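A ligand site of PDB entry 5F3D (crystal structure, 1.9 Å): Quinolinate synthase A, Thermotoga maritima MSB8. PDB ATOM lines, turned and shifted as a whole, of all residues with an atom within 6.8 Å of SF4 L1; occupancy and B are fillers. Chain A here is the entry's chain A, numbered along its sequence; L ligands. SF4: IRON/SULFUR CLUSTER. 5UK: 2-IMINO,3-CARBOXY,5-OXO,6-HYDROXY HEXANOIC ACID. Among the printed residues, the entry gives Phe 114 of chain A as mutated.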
ATOM      1  N   HIS A  26      24.021  -7.103  26.004  1.00  0.00           N
ATOM      2  CA  HIS A  26      24.847  -7.929  25.180  1.00  0.00           C
ATOM      3  C   HIS A  26      26.340  -7.602  25.430  1.00  0.00           C
ATOM      4  O   HIS A  26      26.707  -6.457  25.841  1.00  0.00           O
ATOM      5  CB  HIS A  26      24.490  -7.756  23.725  1.00  0.00           C
ATOM      6  CG  HIS A  26      25.182  -8.731  22.826  1.00  0.00           C
ATOM      7  ND1 HIS A  26      26.433  -8.491  22.285  1.00  0.00           N
ATOM      8  CD2 HIS A  26      24.806  -9.950  22.356  1.00  0.00           C
ATOM      9  CE1 HIS A  26      26.791  -9.504  21.522  1.00  0.00           C
ATOM     10  NE2 HIS A  26      25.845 -10.420  21.572  1.00  0.00           N
ATOM     11  N   TYR A  28      28.634  -6.794  23.583  1.00  0.00           N
ATOM     12  CA  TYR A  28      29.245  -5.772  22.744  1.00  0.00           C
ATOM     13  C   TYR A  28      28.816  -4.352  23.173  1.00  0.00           C
ATOM     14  O   TYR A  28      29.169  -3.377  22.537  1.00  0.00           O
ATOM     15  CB  TYR A  28      28.913  -6.024  21.260  1.00  0.00           C
ATOM     16  CG  TYR A  28      29.443  -7.281  20.609  1.00  0.00           C
ATOM     17  CD1 TYR A  28      30.407  -8.078  21.190  1.00  0.00           C
ATOM     18  CD2 TYR A  28      28.976  -7.677  19.363  1.00  0.00           C
ATOM     19  CE1 TYR A  28      30.875  -9.215  20.566  1.00  0.00           C
ATOM     20  CE2 TYR A  28      29.400  -8.826  18.743  1.00  0.00           C
ATOM     21  CZ  TYR A  28      30.347  -9.593  19.355  1.00  0.00           C
ATOM     22  OH  TYR A  28      30.775 -10.705  18.717  1.00  0.00           O
ATOM     23  N   VAL A  63      20.798  -4.905  20.155  1.00  0.00           N
ATOM     24  CA  VAL A  63      20.224  -4.427  18.884  1.00  0.00           C
ATOM     25  C   VAL A  63      18.848  -5.026  18.764  1.00  0.00           C
ATOM     26  O   VAL A  63      18.586  -6.034  19.414  1.00  0.00           O
ATOM     27  CB  VAL A  63      21.100  -4.824  17.681  1.00  0.00           C
ATOM     28  CG1 VAL A  63      22.429  -4.086  17.737  1.00  0.00           C
ATOM     29  CG2 VAL A  63      21.282  -6.328  17.583  1.00  0.00           C
ATOM     30  N   MET A  66      17.567  -8.814  18.646  1.00  0.00           N
ATOM     31  CA  MET A  66      17.751  -9.461  19.933  1.00  0.00           C
ATOM     32  C   MET A  66      16.681  -9.047  20.913  1.00  0.00           C
ATOM     33  O   MET A  66      16.153  -9.910  21.640  1.00  0.00           O
ATOM     34  CB  MET A  66      19.134  -9.142  20.539  1.00  0.00           C
ATOM     35  CG  MET A  66      20.324  -9.656  19.723  1.00  0.00           C
ATOM     36  SD  MET A  66      21.925  -9.030  20.386  1.00  0.00           S
ATOM     37  CE  MET A  66      22.984  -9.679  19.125  1.00  0.00           C
ATOM     38  N   THR A  87      20.280  -1.725  15.287  1.00  0.00           N
ATOM     39  CA  THR A  87      19.964  -2.893  14.521  1.00  0.00           C
ATOM     40  C   THR A  87      21.225  -3.566  13.985  1.00  0.00           C
ATOM     41  O   THR A  87      22.312  -3.111  14.217  1.00  0.00           O
ATOM     42  CB  THR A  87      19.046  -2.519  13.359  1.00  0.00           C
ATOM     43  OG1 THR A  87      18.495  -3.719  12.839  1.00  0.00           O
ATOM     44  CG2 THR A  87      19.807  -1.709  12.233  1.00  0.00           C
ATOM     45  N   CYS A  88      21.065  -4.671  13.250  1.00  0.00           N
ATOM     46  CA  CYS A  88      22.186  -5.344  12.605  1.00  0.00           C
ATOM     47  C   CYS A  88      21.965  -5.207  11.089  1.00  0.00           C
ATOM     48  O   CYS A  88      20.959  -5.690  10.599  1.00  0.00           O
ATOM     49  CB  CYS A  88      22.279  -6.818  13.008  1.00  0.00           C
ATOM     50  SG  CYS A  88      23.525  -7.736  12.046  1.00  0.00           S
ATOM     51  N   PRO A  89      22.881  -4.534  10.364  1.00  0.00           N
ATOM     52  CA  PRO A  89      22.698  -4.303   8.927  1.00  0.00           C
ATOM     53  C   PRO A  89      22.720  -5.533   8.049  1.00  0.00           C
ATOM     54  O   PRO A  89      22.197  -5.482   6.953  1.00  0.00           O
ATOM     55  CB  PRO A  89      23.867  -3.378   8.564  1.00  0.00           C
ATOM     56  CG  PRO A  89      24.151  -2.654   9.844  1.00  0.00           C
ATOM     57  CD  PRO A  89      23.997  -3.721  10.884  1.00  0.00           C
ATOM     58  N   MET A  90      23.343  -6.600   8.547  1.00  0.00           N
ATOM     59  CA  MET A  90      23.414  -7.858   7.818  1.00  0.00           C
ATOM     60  C   MET A  90      22.018  -8.461   7.568  1.00  0.00           C
ATOM     61  O   MET A  90      21.752  -8.979   6.490  1.00  0.00           O
ATOM     62  CB  MET A  90      24.261  -8.847   8.621  1.00  0.00           C
ATOM     63  CG  MET A  90      24.568 -10.159   7.923  1.00  0.00           C
ATOM     64  SD  MET A  90      25.769 -11.115   8.866  1.00  0.00           S
ATOM     65  CE  MET A  90      24.862 -11.474  10.384  1.00  0.00           C
ATOM     66  N   ALA A  91      21.140  -8.369   8.551  1.00  0.00           N
ATOM     67  CA  ALA A  91      19.794  -8.957   8.463  1.00  0.00           C
ATOM     68  C   ALA A  91      18.967  -8.454   7.298  1.00  0.00           C
ATOM     69  O   ALA A  91      18.254  -9.199   6.639  1.00  0.00           O
ATOM     70  CB  ALA A  91      19.047  -8.670   9.735  1.00  0.00           C
ATOM     71  N   PHE A 114      19.710 -17.269  11.603  1.00  0.00           N
ATOM     72  CA  PHE A 114      20.571 -16.743  12.659  1.00  0.00           C
ATOM     73  C   PHE A 114      19.754 -15.680  13.388  1.00  0.00           C
ATOM     74  O   PHE A 114      18.827 -15.071  12.828  1.00  0.00           O
ATOM     75  CB  PHE A 114      21.848 -16.220  11.958  1.00  0.00           C
ATOM     76  CG  PHE A 114      22.888 -15.624  12.860  1.00  0.00           C
ATOM     77  CD1 PHE A 114      23.533 -16.392  13.804  1.00  0.00           C
ATOM     78  CD2 PHE A 114      23.315 -14.296  12.668  1.00  0.00           C
ATOM     79  CE1 PHE A 114      24.539 -15.834  14.596  1.00  0.00           C
ATOM     80  CE2 PHE A 114      24.311 -13.728  13.450  1.00  0.00           C
ATOM     81  CZ  PHE A 114      24.929 -14.506  14.424  1.00  0.00           C
ATOM     82  N   ASN A 116      20.198 -12.689  14.147  1.00  0.00           N
ATOM     83  CA  ASN A 116      20.165 -11.385  13.526  1.00  0.00           C
ATOM     84  C   ASN A 116      19.496 -11.516  12.195  1.00  0.00           C
ATOM     85  O   ASN A 116      20.131 -11.540  11.139  1.00  0.00           O
ATOM     86  CB  ASN A 116      21.578 -10.776  13.383  1.00  0.00           C
ATOM     87  CG  ASN A 116      22.073 -10.166  14.689  1.00  0.00           C
ATOM     88  OD1 ASN A 116      21.288  -9.866  15.602  1.00  0.00           O
ATOM     89  ND2 ASN A 116      23.401  -9.948  14.781  1.00  0.00           N
ATOM     90  N   ASP A 151      24.218 -14.990   7.649  1.00  0.00           N
ATOM     91  CA  ASP A 151      25.704 -14.853   7.682  1.00  0.00           C
ATOM     92  C   ASP A 151      26.367 -16.011   6.926  1.00  0.00           C
ATOM     93  O   ASP A 151      26.295 -17.162   7.350  1.00  0.00           O
ATOM     94  CB  ASP A 151      26.234 -14.758   9.129  1.00  0.00           C
ATOM     95  CG  ASP A 151      27.731 -14.358   9.188  1.00  0.00           C
ATOM     96  OD1 ASP A 151      28.575 -15.202   8.876  1.00  0.00           O
ATOM     97  OD2 ASP A 151      28.058 -13.205   9.556  1.00  0.00           O
ATOM     98  N   HIS A 174      27.307 -10.887   5.504  1.00  0.00           N
ATOM     99  CA  HIS A 174      28.542 -10.875   6.306  1.00  0.00           C
ATOM    100  C   HIS A 174      28.512  -9.745   7.339  1.00  0.00           C
ATOM    101  O   HIS A 174      27.840  -8.730   7.136  1.00  0.00           O
ATOM    102  CB  HIS A 174      29.761 -10.678   5.393  1.00  0.00           C
ATOM    103  CG  HIS A 174      29.879  -9.283   4.884  1.00  0.00           C
ATOM    104  ND1 HIS A 174      28.914  -8.722   4.071  1.00  0.00           N
ATOM    105  CD2 HIS A 174      30.769  -8.305   5.174  1.00  0.00           C
ATOM    106  CE1 HIS A 174      29.235  -7.457   3.844  1.00  0.00           C
ATOM    107  NE2 HIS A 174      30.349  -7.183   4.509  1.00  0.00           N
ATOM    108  N   CYS A 175      29.239  -9.957   8.429  1.00  0.00           N
ATOM    109  CA  CYS A 175      29.380  -8.952   9.501  1.00  0.00           C
ATOM    110  C   CYS A 175      30.679  -8.147   9.313  1.00  0.00           C
ATOM    111  O   CYS A 175      31.760  -8.725   9.459  1.00  0.00           O
ATOM    112  CB  CYS A 175      29.431  -9.645  10.852  1.00  0.00           C
ATOM    113  SG  CYS A 175      29.966  -8.549  12.181  1.00  0.00           S
ATOM    114  N   PRO A 176      30.571  -6.820   9.033  1.00  0.00           N
ATOM    115  CA  PRO A 176      31.771  -5.952   8.766  1.00  0.00           C
ATOM    116  C   PRO A 176      32.744  -5.906   9.947  1.00  0.00           C
ATOM    117  O   PRO A 176      33.949  -5.794   9.786  1.00  0.00           O
ATOM    118  CB  PRO A 176      31.178  -4.559   8.499  1.00  0.00           C
ATOM    119  CG  PRO A 176      29.747  -4.612   8.899  1.00  0.00           C
ATOM    120  CD  PRO A 176      29.303  -6.052   8.988  1.00  0.00           C
ATOM    121  N   VAL A 177      32.198  -6.053  11.144  1.00  0.00           N
ATOM    122  CA  VAL A 177      32.979  -6.034  12.338  1.00  0.00           C
ATOM    123  C   VAL A 177      34.022  -7.164  12.347  1.00  0.00           C
ATOM    124  O   VAL A 177      35.131  -6.961  12.825  1.00  0.00           O
ATOM    125  CB  VAL A 177      32.045  -6.084  13.581  1.00  0.00           C
ATOM    126  CG1 VAL A 177      32.827  -5.809  14.857  1.00  0.00           C
ATOM    127  CG2 VAL A 177      30.912  -5.063  13.426  1.00  0.00           C
ATOM    128  N   HIS A 178      33.693  -8.334  11.804  1.00  0.00           N
ATOM    129  CA  HIS A 178      34.534  -9.543  11.964  1.00  0.00           C
ATOM    130  C   HIS A 178      35.435  -9.830  10.767  1.00  0.00           C
ATOM    131  O   HIS A 178      36.018 -10.919  10.649  1.00  0.00           O
ATOM    132  CB  HIS A 178      33.648 -10.762  12.291  1.00  0.00           C
ATOM    133  CG  HIS A 178      33.136 -10.769  13.686  1.00  0.00           C
ATOM    134  ND1 HIS A 178      31.892 -10.296  14.031  1.00  0.00           N
ATOM    135  CD2 HIS A 178      33.731 -11.130  14.847  1.00  0.00           C
ATOM    136  CE1 HIS A 178      31.739 -10.394  15.336  1.00  0.00           C
ATOM    137  NE2 HIS A 178      32.836 -10.905  15.855  1.00  0.00           N
ATOM    138  N   GLU A 202      32.126 -15.866  12.616  1.00  0.00           N
ATOM    139  CA  GLU A 202      31.795 -14.871  11.582  1.00  0.00           C
ATOM    140  C   GLU A 202      33.033 -14.313  10.864  1.00  0.00           C
ATOM    141  O   GLU A 202      32.902 -13.668   9.804  1.00  0.00           O
ATOM    142  CB  GLU A 202      30.977 -13.713  12.169  1.00  0.00           C
ATOM    143  CG  GLU A 202      29.546 -14.089  12.466  1.00  0.00           C
ATOM    144  CD  GLU A 202      28.807 -13.050  13.283  1.00  0.00           C
ATOM    145  OE1 GLU A 202      29.225 -11.850  13.315  1.00  0.00           O
ATOM    146  OE2 GLU A 202      27.820 -13.446  13.938  1.00  0.00           O
ATOM    147  N   THR A 236      37.037 -10.532  18.040  1.00  0.00           N
ATOM    148  CA  THR A 236      35.624 -10.151  17.964  1.00  0.00           C
ATOM    149  C   THR A 236      35.532  -8.674  18.251  1.00  0.00           C
ATOM    150  O   THR A 236      36.568  -7.996  18.322  1.00  0.00           O
ATOM    151  CB  THR A 236      34.733 -11.047  18.876  1.00  0.00           C
ATOM    152  OG1 THR A 236      33.363 -10.932  18.466  1.00  0.00           O
ATOM    153  CG2 THR A 236      34.852 -10.665  20.363  1.00  0.00           C
ATOM    154  N   GLU A 237      34.309  -8.185  18.441  1.00  0.00           N
ATOM    155  CA  GLU A 237      33.993  -6.798  18.709  1.00  0.00           C
ATOM    156  C   GLU A 237      34.536  -6.429  20.086  1.00  0.00           C
ATOM    157  O   GLU A 237      34.565  -7.261  21.016  1.00  0.00           O
ATOM    158  CB  GLU A 237      32.478  -6.562  18.600  1.00  0.00           C
ATOM    159  CG  GLU A 237      32.017  -5.157  18.306  1.00  0.00           C
ATOM    160  CD  GLU A 237      31.932  -4.280  19.523  1.00  0.00           C
ATOM    161  OE1 GLU A 237      32.037  -4.782  20.649  1.00  0.00           O
ATOM    162  OE2 GLU A 237      31.731  -3.059  19.348  1.00  0.00           O
ATOM    163  N   VAL A 260      34.625  -2.296  16.080  1.00  0.00           N
ATOM    164  CA  VAL A 260      33.569  -1.640  16.795  1.00  0.00           C
ATOM    165  C   VAL A 260      32.310  -1.874  15.963  1.00  0.00           C
ATOM    166  O   VAL A 260      32.323  -1.692  14.744  1.00  0.00           O
ATOM    167  CB  VAL A 260      33.854  -0.130  16.956  1.00  0.00           C
ATOM    168  CG1 VAL A 260      32.712   0.579  17.706  1.00  0.00           C
ATOM    169  CG2 VAL A 260      35.165   0.062  17.687  1.00  0.00           C
ATOM    170  N   CYS A 261      31.229  -2.273  16.622  1.00  0.00           N
ATOM    171  CA  CYS A 261      29.918  -2.355  15.968  1.00  0.00           C
ATOM    172  C   CYS A 261      29.209  -1.037  16.279  1.00  0.00           C
ATOM    173  O   CYS A 261      28.822  -0.796  17.431  1.00  0.00           O
ATOM    174  CB  CYS A 261      29.066  -3.503  16.514  1.00  0.00           C
ATOM    175  SG  CYS A 261      27.434  -3.544  15.749  1.00  0.00           S
ATOM    176  N   VAL A 262      28.989  -0.221  15.266  1.00  0.00           N
ATOM    177  CA  VAL A 262      28.370   1.133  15.431  1.00  0.00           C
ATOM    178  C   VAL A 262      26.980   0.995  16.045  1.00  0.00           C
ATOM    179  O   VAL A 262      26.613   1.686  16.990  1.00  0.00           O
ATOM    180  CB  VAL A 262      28.342   1.893  14.073  1.00  0.00           C
ATOM    181  CG1 VAL A 262      27.494   3.172  14.134  1.00  0.00           C
ATOM    182  CG2 VAL A 262      29.776   2.238  13.633  1.00  0.00           C
ATOM    183  N   ASN A 263      26.195   0.046  15.544  1.00  0.00           N
ATOM    184  CA  ASN A 263      24.863  -0.181  16.177  1.00  0.00           C
ATOM    185  C   ASN A 263      24.849  -0.510  17.673  1.00  0.00           C
ATOM    186  O   ASN A 263      24.094   0.092  18.474  1.00  0.00           O
ATOM    187  CB  ASN A 263      24.085  -1.172  15.336  1.00  0.00           C
ATOM    188  CG  ASN A 263      23.381  -0.459  14.186  1.00  0.00           C
ATOM    189  OD1 ASN A 263      22.319   0.129  14.389  1.00  0.00           O
ATOM    190  ND2 ASN A 263      23.964  -0.500  13.010  1.00  0.00           N
ATOM    191  N   MET A 264      25.712  -1.433  18.072  1.00  0.00           N
ATOM    192  CA  MET A 264      25.848  -1.781  19.458  1.00  0.00           C
ATOM    193  C   MET A 264      26.253  -0.588  20.312  1.00  0.00           C
ATOM    194  O   MET A 264      25.821  -0.445  21.451  1.00  0.00           O
ATOM    195  CB  MET A 264      26.885  -2.899  19.613  1.00  0.00           C
ATOM    196  CG  MET A 264      26.380  -4.256  19.170  1.00  0.00           C
ATOM    197  SD  MET A 264      25.183  -4.893  20.372  1.00  0.00           S
ATOM    198  CE  MET A 264      24.908  -6.562  19.815  1.00  0.00           C
HETATM  199 FE1  SF4 L   1      28.157  -7.705  13.368  1.00  0.00          FE
HETATM  200 FE2  SF4 L   1      27.014  -5.614  14.754  1.00  0.00          FE
HETATM  201 FE3  SF4 L   1      26.608  -8.363  15.537  1.00  0.00          FE
HETATM  202 FE4  SF4 L   1      25.360  -7.325  13.345  1.00  0.00          FE
HETATM  203  S1  SF4 L   1      24.974  -6.675  15.434  1.00  0.00           S
HETATM  204  S2  SF4 L   1      26.613  -9.398  13.478  1.00  0.00           S
HETATM  205  S3  SF4 L   1      27.013  -5.816  12.513  1.00  0.00           S
HETATM  206  S4  SF4 L   1      28.680  -7.108  15.498  1.00  0.00           S
HETATM  207  OAC 5UK L   2      24.629 -15.451  18.523  1.00  0.00           O
HETATM  208  CAJ 5UK L   2      25.586 -15.002  19.157  1.00  0.00           C
HETATM  209  OAE 5UK L   2      26.397 -15.748  19.707  1.00  0.00           O
HETATM  210  CAL 5UK L   2      25.750 -13.581  19.239  1.00  0.00           C
HETATM  211  NAA 5UK L   2      24.724 -13.039  19.693  1.00  0.00           N
HETATM  212  CAN 5UK L   2      27.040 -12.806  18.996  1.00  0.00           C
HETATM  213  CAK 5UK L   2      28.005 -13.537  19.838  1.00  0.00           C
HETATM  214  OAF 5UK L   2      29.037 -14.110  19.441  1.00  0.00           O
HETATM  215  OAD 5UK L   2      27.690 -13.546  20.993  1.00  0.00           O
HETATM  216  CAI 5UK L   2      27.617 -12.585  17.589  1.00  0.00           C
HETATM  217  CAM 5UK L   2      26.802 -11.710  16.672  1.00  0.00           C
HETATM  218  CAH 5UK L   2      25.692 -10.798  17.085  1.00  0.00           C
HETATM  219  OAB 5UK L   2      26.163  -9.461  17.215  1.00  0.00           O
HETATM  220  OAG 5UK L   2      27.030 -11.742  15.495  1.00  0.00           O
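OAB of 5UK L2 binds FE3 of SF4 L1, at 2.1 Å.
ND2 of Asn 116 sits close to SG of Cys 88 (3.5 Å).
The backbone NH (N) of Met 90 sits close to the side-chain sulfur (SG) of Cys 88 (3.7 Å).
SD of Met 90 is in hydrogen-bond range of N of Cys 175 (3.7 Å).
The side-chain sulfur (SG) of Cys 261 sits close to the backbone NH (N) of Met 264 (3.6 Å).
N of Cys 261 sits at hydrogen-bond distance from OE2 of Glu 237 (2.9 Å).
The side-chain carboxylate (OE1) of Glu 202 lies within hydrogen-bond range of a ring nitrogen (ND1) of His 178 (3.2 Å).
N of Tyr 28 sits close to ND1 of His 26 (3.1 Å).
OH of Tyr 28 is in hydrogen-bond range of OG1 of Thr 236, 2.6 Å away.
OE1 of Glu 202 sits close to S2 of SF4 L1, at 3.6 Å.
Tyr 28 touches SF4 L1 (CE2 to S4, 3.7 Å).
Val 177 touches SF4 L1.
Hydrophobic or aromatic side chains within 4 Å of SF4 L1: Tyr 28 and Val 177.
Seven residues have an atom within 4 Å of SF4 L1: Tyr 28, Cys 88, Asn 116, Cys 175, Val 177, Glu 202 and Cys 261.
The nearest printed residue that does not touch SF4 L1 is Pro 89 (4.02 Å).
The side-chain sulfur (SG) of Cys 88 is bound to an iron atom (FE4) of SF4 L1, at 2.3 Å.
An iron atom (FE1) of SF4 L1 is bound by the side-chain sulfur (SG) of Cys 175, at 2.3 Å.
An iron atom (FE2) of SF4 L1 is bound by the side-chain sulfur (SG) of Cys 261 (2.3 Å).
ND2 of Asn 116 sits close to S2 of SF4 L1, 3.5 Å away.
The side-chain carboxylate (OE2) of Glu 202 sits close to an oxygen (OAG) of 5UK L2, at 2.4 Å.
NAA of 5UK L2 is in hydrogen-bond range of NE2 of His 26 (3.4 Å).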
